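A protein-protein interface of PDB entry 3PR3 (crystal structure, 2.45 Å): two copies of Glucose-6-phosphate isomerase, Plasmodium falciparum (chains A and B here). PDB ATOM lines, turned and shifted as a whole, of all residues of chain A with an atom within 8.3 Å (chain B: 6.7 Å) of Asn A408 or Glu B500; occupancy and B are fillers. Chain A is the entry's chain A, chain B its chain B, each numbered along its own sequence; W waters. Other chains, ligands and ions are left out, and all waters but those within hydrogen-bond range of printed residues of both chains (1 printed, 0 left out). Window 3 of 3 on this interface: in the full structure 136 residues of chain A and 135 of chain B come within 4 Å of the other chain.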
ATOM      1  N   ASN A  20     -28.121  18.580 -19.297  1.00  0.00           N
ATOM      2  CA  ASN A  20     -29.479  19.086 -19.532  1.00  0.00           C
ATOM      3  C   ASN A  20     -30.465  17.890 -19.694  1.00  0.00           C
ATOM      4  O   ASN A  20     -31.613  17.943 -19.232  1.00  0.00           O
ATOM      5  CB  ASN A  20     -29.494  20.085 -20.696  1.00  0.00           C
ATOM      6  N   MET A 105     -20.943  20.223  -5.186  1.00  0.00           N
ATOM      7  CA  MET A 105     -21.180  21.324  -6.109  1.00  0.00           C
ATOM      8  C   MET A 105     -22.061  22.461  -5.635  1.00  0.00           C
ATOM      9  O   MET A 105     -21.847  23.588  -6.067  1.00  0.00           O
ATOM     10  CB  MET A 105     -21.605  20.784  -7.483  1.00  0.00           C
ATOM     11  CG  MET A 105     -20.428  20.250  -8.274  1.00  0.00           C
ATOM     12  SD  MET A 105     -20.824  19.651  -9.932  1.00  0.00           S
ATOM     13  CE  MET A 105     -19.148  19.317 -10.527  1.00  0.00           C
ATOM     14  N   THR A 106     -23.034  22.200  -4.752  1.00  0.00           N
ATOM     15  CA  THR A 106     -23.911  23.282  -4.251  1.00  0.00           C
ATOM     16  C   THR A 106     -23.269  24.114  -3.129  1.00  0.00           C
ATOM     17  O   THR A 106     -23.700  25.245  -2.864  1.00  0.00           O
ATOM     18  CB  THR A 106     -25.297  22.760  -3.869  1.00  0.00           C
ATOM     19  OG1 THR A 106     -25.182  21.988  -2.679  1.00  0.00           O
ATOM     20  CG2 THR A 106     -25.935  21.937  -4.971  1.00  0.00           C
ATOM     21  N   GLU A 107     -22.251  23.556  -2.466  1.00  0.00           N
ATOM     22  CA  GLU A 107     -21.547  24.250  -1.390  1.00  0.00           C
ATOM     23  C   GLU A 107     -20.091  24.538  -1.780  1.00  0.00           C
ATOM     24  O   GLU A 107     -19.346  25.160  -1.012  1.00  0.00           O
ATOM     25  CB  GLU A 107     -21.628  23.447  -0.074  1.00  0.00           C
ATOM     26  CG  GLU A 107     -23.043  23.196   0.396  1.00  0.00           C
ATOM     27  CD  GLU A 107     -23.125  22.525   1.749  1.00  0.00           C
ATOM     28  OE1 GLU A 107     -22.538  21.429   1.916  1.00  0.00           O
ATOM     29  OE2 GLU A 107     -23.794  23.094   2.642  1.00  0.00           O
ATOM     30  N   SER A 403     -34.178  16.262  -4.593  1.00  0.00           N
ATOM     31  CA  SER A 403     -35.159  16.646  -5.615  1.00  0.00           C
ATOM     32  C   SER A 403     -34.535  17.279  -6.852  1.00  0.00           C
ATOM     33  O   SER A 403     -35.234  17.490  -7.844  1.00  0.00           O
ATOM     34  CB  SER A 403     -36.121  17.668  -5.007  1.00  0.00           C
ATOM     35  OG  SER A 403     -35.397  18.707  -4.351  1.00  0.00           O
ATOM     36  N   VAL A 404     -33.266  17.688  -6.763  1.00  0.00           N
ATOM     37  CA  VAL A 404     -32.549  18.419  -7.821  1.00  0.00           C
ATOM     38  C   VAL A 404     -31.259  17.675  -8.208  1.00  0.00           C
ATOM     39  O   VAL A 404     -30.533  17.222  -7.330  1.00  0.00           O
ATOM     40  CB  VAL A 404     -32.299  19.892  -7.368  1.00  0.00           C
ATOM     41  CG1 VAL A 404     -31.581  20.697  -8.437  1.00  0.00           C
ATOM     42  CG2 VAL A 404     -33.602  20.580  -7.002  1.00  0.00           C
ATOM     43  N   ASP A 405     -31.002  17.520  -9.522  1.00  0.00           N
ATOM     44  CA  ASP A 405     -29.837  16.778 -10.001  1.00  0.00           C
ATOM     45  C   ASP A 405     -28.532  17.559  -9.937  1.00  0.00           C
ATOM     46  O   ASP A 405     -28.534  18.723  -9.536  1.00  0.00           O
ATOM     47  CB  ASP A 405     -30.098  16.100 -11.372  1.00  0.00           C
ATOM     48  CG  ASP A 405     -30.128  16.978 -12.624  1.00  0.00           C
ATOM     49  OD1 ASP A 405     -29.713  18.156 -12.542  1.00  0.00           O
ATOM     50  OD2 ASP A 405     -30.507  16.462 -13.704  1.00  0.00           O
ATOM     51  N   ARG A 406     -27.410  16.922 -10.318  1.00  0.00           N
ATOM     52  CA  ARG A 406     -26.100  17.565 -10.312  1.00  0.00           C
ATOM     53  C   ARG A 406     -25.970  18.687 -11.373  1.00  0.00           C
ATOM     54  O   ARG A 406     -25.111  19.557 -11.227  1.00  0.00           O
ATOM     55  CB  ARG A 406     -24.975  16.520 -10.379  1.00  0.00           C
ATOM     56  CG  ARG A 406     -24.583  15.977  -8.991  1.00  0.00           C
ATOM     57  CD  ARG A 406     -23.654  14.766  -9.005  1.00  0.00           C
ATOM     58  NE  ARG A 406     -22.589  14.843 -10.019  1.00  0.00           N
ATOM     59  CZ  ARG A 406     -21.370  15.338  -9.813  1.00  0.00           C
ATOM     60  NH1 ARG A 406     -21.029  15.810  -8.619  1.00  0.00           N
ATOM     61  NH2 ARG A 406     -20.484  15.360 -10.797  1.00  0.00           N
ATOM     62  N   ASN A 407     -26.875  18.708 -12.384  1.00  0.00           N
ATOM     63  CA  ASN A 407     -26.930  19.758 -13.411  1.00  0.00           C
ATOM     64  C   ASN A 407     -27.886  20.885 -12.926  1.00  0.00           C
ATOM     65  O   ASN A 407     -28.298  21.741 -13.717  1.00  0.00           O
ATOM     66  CB  ASN A 407     -27.399  19.207 -14.779  1.00  0.00           C
ATOM     67  CG  ASN A 407     -26.799  17.889 -15.236  1.00  0.00           C
ATOM     68  OD1 ASN A 407     -25.577  17.693 -15.232  1.00  0.00           O
ATOM     69  ND2 ASN A 407     -27.660  16.971 -15.706  1.00  0.00           N
ATOM     70  N   ASN A 408     -28.239  20.859 -11.618  1.00  0.00           N
ATOM     71  CA  ASN A 408     -29.120  21.800 -10.917  1.00  0.00           C
ATOM     72  C   ASN A 408     -30.545  21.845 -11.433  1.00  0.00           C
ATOM     73  O   ASN A 408     -31.278  22.828 -11.190  1.00  0.00           O
ATOM     74  CB  ASN A 408     -28.535  23.192 -10.816  1.00  0.00           C
ATOM     75  CG  ASN A 408     -27.089  23.212 -10.469  1.00  0.00           C
ATOM     76  OD1 ASN A 408     -26.267  23.634 -11.269  1.00  0.00           O
ATOM     77  ND2 ASN A 408     -26.727  22.691  -9.324  1.00  0.00           N
ATOM     78  N   GLN A 409     -30.946  20.754 -12.087  1.00  0.00           N
ATOM     79  CA  GLN A 409     -32.271  20.594 -12.674  1.00  0.00           C
ATOM     80  C   GLN A 409     -33.210  19.866 -11.724  1.00  0.00           C
ATOM     81  O   GLN A 409     -32.845  18.782 -11.266  1.00  0.00           O
ATOM     82  CB  GLN A 409     -32.198  19.823 -14.009  1.00  0.00           C
ATOM     83  CG  GLN A 409     -31.075  20.273 -14.946  1.00  0.00           C
ATOM     84  CD  GLN A 409     -31.256  19.767 -16.350  1.00  0.00           C
ATOM     85  OE1 GLN A 409     -31.447  20.548 -17.284  1.00  0.00           O
ATOM     86  NE2 GLN A 409     -31.234  18.453 -16.523  1.00  0.00           N
ATOM     87  N   PRO A 410     -34.420  20.418 -11.427  1.00  0.00           N
ATOM     88  CA  PRO A 410     -35.373  19.660 -10.576  1.00  0.00           C
ATOM     89  C   PRO A 410     -35.699  18.327 -11.262  1.00  0.00           C
ATOM     90  O   PRO A 410     -35.872  18.283 -12.482  1.00  0.00           O
ATOM     91  CB  PRO A 410     -36.624  20.574 -10.518  1.00  0.00           C
ATOM     92  CG  PRO A 410     -36.123  21.963 -10.901  1.00  0.00           C
ATOM     93  CD  PRO A 410     -35.005  21.705 -11.889  1.00  0.00           C
ATOM     94  N   ILE A 411     -35.677  17.228 -10.509  1.00  0.00           N
ATOM     95  CA  ILE A 411     -35.928  15.907 -11.095  1.00  0.00           C
ATOM     96  C   ILE A 411     -37.150  15.257 -10.487  1.00  0.00           C
ATOM     97  O   ILE A 411     -37.560  15.627  -9.380  1.00  0.00           O
ATOM     98  CB  ILE A 411     -34.665  14.985 -11.122  1.00  0.00           C
ATOM     99  CG1 ILE A 411     -33.975  14.865  -9.745  1.00  0.00           C
ATOM    100  CG2 ILE A 411     -33.685  15.429 -12.231  1.00  0.00           C
ATOM    101  CD1 ILE A 411     -34.654  13.889  -8.759  1.00  0.00           C
ATOM    102  N   ASN A 545     -27.409  10.715  -9.857  1.00  0.00           N
ATOM    103  CA  ASN A 545     -26.964  12.012 -10.349  1.00  0.00           C
ATOM    104  C   ASN A 545     -27.443  13.166  -9.485  1.00  0.00           C
ATOM    105  O   ASN A 545     -27.967  14.164  -9.976  1.00  0.00           O
ATOM    106  CB  ASN A 545     -27.312  12.210 -11.825  1.00  0.00           C
ATOM    107  CG  ASN A 545     -26.569  13.339 -12.501  1.00  0.00           C
ATOM    108  OD1 ASN A 545     -25.375  13.547 -12.298  1.00  0.00           O
ATOM    109  ND2 ASN A 545     -27.258  14.076 -13.337  1.00  0.00           N
ATOM    110  N   ILE A 546     -27.256  13.031  -8.191  1.00  0.00           N
ATOM    111  CA  ILE A 546     -27.624  14.036  -7.198  1.00  0.00           C
ATOM    112  C   ILE A 546     -26.410  14.338  -6.317  1.00  0.00           C
ATOM    113  O   ILE A 546     -25.389  13.620  -6.366  1.00  0.00           O
ATOM    114  CB  ILE A 546     -28.823  13.543  -6.339  1.00  0.00           C
ATOM    115  CG1 ILE A 546     -28.499  12.177  -5.672  1.00  0.00           C
ATOM    116  CG2 ILE A 546     -30.119  13.516  -7.159  1.00  0.00           C
ATOM    117  CD1 ILE A 546     -29.323  11.795  -4.560  1.00  0.00           C
ATOM    118  N   ASN A 547     -26.535  15.397  -5.499  1.00  0.00           N
ATOM    119  CA  ASN A 547     -25.512  15.768  -4.549  1.00  0.00           C
ATOM    120  C   ASN A 547     -25.838  15.064  -3.250  1.00  0.00           C
ATOM    121  O   ASN A 547     -26.826  15.395  -2.600  1.00  0.00           O
ATOM    122  CB  ASN A 547     -25.434  17.283  -4.353  1.00  0.00           C
ATOM    123  CG  ASN A 547     -24.217  17.728  -3.569  1.00  0.00           C
ATOM    124  OD1 ASN A 547     -23.319  16.949  -3.243  1.00  0.00           O
ATOM    125  ND2 ASN A 547     -24.172  18.992  -3.231  1.00  0.00           N
ATOM    126  N   ASP A 550     -24.849  17.702   0.370  1.00  0.00           N
ATOM    127  CA  ASP A 550     -25.533  18.865   0.945  1.00  0.00           C
ATOM    128  C   ASP A 550     -26.796  18.442   1.720  1.00  0.00           C
ATOM    129  O   ASP A 550     -27.124  17.248   1.749  1.00  0.00           O
ATOM    130  CB  ASP A 550     -25.851  19.890  -0.153  1.00  0.00           C
ATOM    131  CG  ASP A 550     -26.758  19.399  -1.272  1.00  0.00           C
ATOM    132  OD1 ASP A 550     -27.283  18.256  -1.171  1.00  0.00           O
ATOM    133  OD2 ASP A 550     -26.921  20.131  -2.262  1.00  0.00           O
ATOM    134  N   TYR B 485     -39.702  29.002  -5.802  1.00  0.00           N
ATOM    135  CA  TYR B 485     -38.511  29.485  -6.500  1.00  0.00           C
ATOM    136  C   TYR B 485     -38.435  31.015  -6.399  1.00  0.00           C
ATOM    137  O   TYR B 485     -37.346  31.559  -6.176  1.00  0.00           O
ATOM    138  CB  TYR B 485     -38.516  29.054  -7.987  1.00  0.00           C
ATOM    139  CG  TYR B 485     -37.236  29.421  -8.701  1.00  0.00           C
ATOM    140  CD1 TYR B 485     -36.091  28.636  -8.571  1.00  0.00           C
ATOM    141  CD2 TYR B 485     -37.141  30.596  -9.443  1.00  0.00           C
ATOM    142  CE1 TYR B 485     -34.889  28.998  -9.176  1.00  0.00           C
ATOM    143  CE2 TYR B 485     -35.937  30.979 -10.046  1.00  0.00           C
ATOM    144  CZ  TYR B 485     -34.816  30.163  -9.927  1.00  0.00           C
ATOM    145  OH  TYR B 485     -33.624  30.520 -10.524  1.00  0.00           O
ATOM    146  N   MET B 497     -26.037  33.698  -3.793  1.00  0.00           N
ATOM    147  CA  MET B 497     -25.658  32.350  -4.223  1.00  0.00           C
ATOM    148  C   MET B 497     -25.650  32.399  -5.767  1.00  0.00           C
ATOM    149  O   MET B 497     -26.391  33.203  -6.352  1.00  0.00           O
ATOM    150  CB  MET B 497     -26.715  31.333  -3.747  1.00  0.00           C
ATOM    151  CG  MET B 497     -26.261  29.868  -3.793  1.00  0.00           C
ATOM    152  SD  MET B 497     -27.635  28.723  -3.432  1.00  0.00           S
ATOM    153  CE  MET B 497     -26.749  27.270  -2.980  1.00  0.00           C
ATOM    154  N   SER B 498     -24.792  31.582  -6.417  1.00  0.00           N
ATOM    155  CA  SER B 498     -24.716  31.483  -7.879  1.00  0.00           C
ATOM    156  C   SER B 498     -26.139  31.113  -8.330  1.00  0.00           C
ATOM    157  O   SER B 498     -26.671  30.116  -7.834  1.00  0.00           O
ATOM    158  CB  SER B 498     -23.704  30.420  -8.291  1.00  0.00           C
ATOM    159  OG  SER B 498     -23.276  30.612  -9.629  1.00  0.00           O
ATOM    160  N   PRO B 499     -26.837  31.989  -9.104  1.00  0.00           N
ATOM    161  CA  PRO B 499     -28.271  31.761  -9.382  1.00  0.00           C
ATOM    162  C   PRO B 499     -28.734  30.387  -9.845  1.00  0.00           C
ATOM    163  O   PRO B 499     -29.874  30.024  -9.555  1.00  0.00           O
ATOM    164  CB  PRO B 499     -28.647  32.894 -10.357  1.00  0.00           C
ATOM    165  CG  PRO B 499     -27.369  33.514 -10.765  1.00  0.00           C
ATOM    166  CD  PRO B 499     -26.393  33.277  -9.674  1.00  0.00           C
ATOM    167  N   GLU B 500     -27.868  29.623 -10.529  1.00  0.00           N
ATOM    168  CA  GLU B 500     -28.213  28.287 -11.026  1.00  0.00           C
ATOM    169  C   GLU B 500     -28.443  27.251  -9.915  1.00  0.00           C
ATOM    170  O   GLU B 500     -29.110  26.244 -10.156  1.00  0.00           O
ATOM    171  CB  GLU B 500     -27.206  27.788 -12.102  1.00  0.00           C
ATOM    172  CG  GLU B 500     -25.881  27.260 -11.568  1.00  0.00           C
ATOM    173  CD  GLU B 500     -24.788  28.277 -11.284  1.00  0.00           C
ATOM    174  OE1 GLU B 500     -25.071  29.498 -11.279  1.00  0.00           O
ATOM    175  OE2 GLU B 500     -23.636  27.841 -11.058  1.00  0.00           O
ATOM    176  N   LEU B 501     -27.903  27.520  -8.710  1.00  0.00           N
ATOM    177  CA  LEU B 501     -27.991  26.663  -7.526  1.00  0.00           C
ATOM    178  C   LEU B 501     -29.283  26.863  -6.689  1.00  0.00           C
ATOM    179  O   LEU B 501     -29.551  26.081  -5.772  1.00  0.00           O
ATOM    180  CB  LEU B 501     -26.752  26.900  -6.628  1.00  0.00           C
ATOM    181  CG  LEU B 501     -25.330  26.679  -7.214  1.00  0.00           C
ATOM    182  CD1 LEU B 501     -24.277  26.959  -6.161  1.00  0.00           C
ATOM    183  CD2 LEU B 501     -25.136  25.253  -7.751  1.00  0.00           C
ATOM    184  N   LEU B 502     -30.076  27.910  -7.003  1.00  0.00           N
ATOM    185  CA  LEU B 502     -31.299  28.247  -6.272  1.00  0.00           C
ATOM    186  C   LEU B 502     -32.385  27.177  -6.259  1.00  0.00           C
ATOM    187  O   LEU B 502     -33.149  27.083  -5.291  1.00  0.00           O
ATOM    188  CB  LEU B 502     -31.854  29.619  -6.682  1.00  0.00           C
ATOM    189  CG  LEU B 502     -30.955  30.841  -6.424  1.00  0.00           C
ATOM    190  CD1 LEU B 502     -31.649  32.122  -6.905  1.00  0.00           C
ATOM    191  CD2 LEU B 502     -30.561  30.953  -4.953  1.00  0.00           C
ATOM    192  N   THR B 503     -32.425  26.341  -7.295  1.00  0.00           N
ATOM    193  CA  THR B 503     -33.393  25.240  -7.398  1.00  0.00           C
ATOM    194  C   THR B 503     -33.295  24.255  -6.215  1.00  0.00           C
ATOM    195  O   THR B 503     -34.302  23.670  -5.828  1.00  0.00           O
ATOM    196  CB  THR B 503     -33.285  24.560  -8.763  1.00  0.00           C
ATOM    197  OG1 THR B 503     -31.927  24.204  -9.015  1.00  0.00           O
ATOM    198  CG2 THR B 503     -33.828  25.443  -9.904  1.00  0.00           C
ATOM    199  N   HIS B 504     -32.088  24.136  -5.600  1.00  0.00           N
ATOM    200  CA  HIS B 504     -31.795  23.257  -4.457  1.00  0.00           C
ATOM    201  C   HIS B 504     -32.474  23.700  -3.176  1.00  0.00           C
ATOM    202  O   HIS B 504     -32.659  22.882  -2.279  1.00  0.00           O
ATOM    203  CB  HIS B 504     -30.280  23.146  -4.238  1.00  0.00           C
ATOM    204  CG  HIS B 504     -29.576  22.496  -5.378  1.00  0.00           C
ATOM    205  ND1 HIS B 504     -29.450  21.128  -5.455  1.00  0.00           N
ATOM    206  CD2 HIS B 504     -29.019  23.048  -6.477  1.00  0.00           C
ATOM    207  CE1 HIS B 504     -28.796  20.890  -6.577  1.00  0.00           C
ATOM    208  NE2 HIS B 504     -28.528  22.017  -7.231  1.00  0.00           N
HETATM  209  O   HOH W   1     -28.984  19.247  -3.622  1.00  0.00           O
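Ser A403 touches none of the printed residues of chain B.
Of the printed residues of chain B, Asp A405 touches His B504.
Of chain B, only Glu B500, Leu B501, Thr B503 and His B504 come within 4 Å of Asn A408.
Of the printed residues of chain A, Met B497 touches Thr A106 (3.7 Å).
Glu B500 touches just one residue of chain A: Asn A408 (3.2 Å).
Printed residues of chain A within 4 Å of Leu B501: Thr A106 (3.8 Å) and Asn A408 (3.4 Å).
The side-chain hydroxyl of Thr A106 lies within hydrogen-bond range of the side-chain amide nitrogen of Asn A547 (3.2 Å).
The side-chain hydroxyl (OG1) of Thr A106 sits at hydrogen-bond distance from the side-chain carboxylate (OD2) of Asp A550.
The side-chain carboxylate (OD1) of Asp A405 is in hydrogen-bond range of the backbone NH (N) of Asn A407 (2.9 Å).
OD1 of Asp A405 is in hydrogen-bond range of N of Asn A408, 3.2 Å away.
OD1 of Asp A405 lies within hydrogen-bond range of N of Gln A409.
The side-chain hydroxyl of Ser B498 is in hydrogen-bond range of the side-chain carboxylate of Glu B500 (2.7 Å).
Met B497 touches Thr A106.
O of Thr A106 touches CD1 of Leu B501, at 3.8 Å.
CG2 of Thr A106 touches NE2 of His B504, at 3.4 Å.
O of Thr B503 touches CG2 of Val A404, 3.4 Å away.
CG1 of Val A404 touches CE1 of His B504 (3.4 Å).
CE1 of His B504 touches O of Asp A405 (3.7 Å).
Glu B500 touches Asn A408 (O to CB, 3.2 Å).
ND2 of Asn A408 touches CD2 of Leu B501, 3.4 Å away.
Water W1 bridges the side-chain carboxylate (OD2) of Asp A550 (2.6 Å) and a ring nitrogen (ND1) of His B504 (2.7 Å).
Of the 9 printed residues of chain B, 5 touch a printed residue of chain A.
Hydrophobic or aromatic side chains of chain B within 4 Å of the printed part of chain A: Met B497, Leu B501 and His B504.
Printed residues of chain A that touch a printed residue of chain B: Thr A106, Val A404, Asp A405 and Asn A408.
Hydrophobic or aromatic side chains of chain A within 4 Å of the printed part of chain B: Val A404.
Among the printed residues, 10 pairs touch across the chains.
The backbone carbonyl oxygen of Asn A408 sits at hydrogen-bond distance from the side-chain hydroxyl of Thr B503 (2.7 Å).
A ring nitrogen (NE2) of His B504 lies within hydrogen-bond range of the side-chain amide nitrogen of Asn A408, at 2.8 Å.
No position is printed for both chains.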
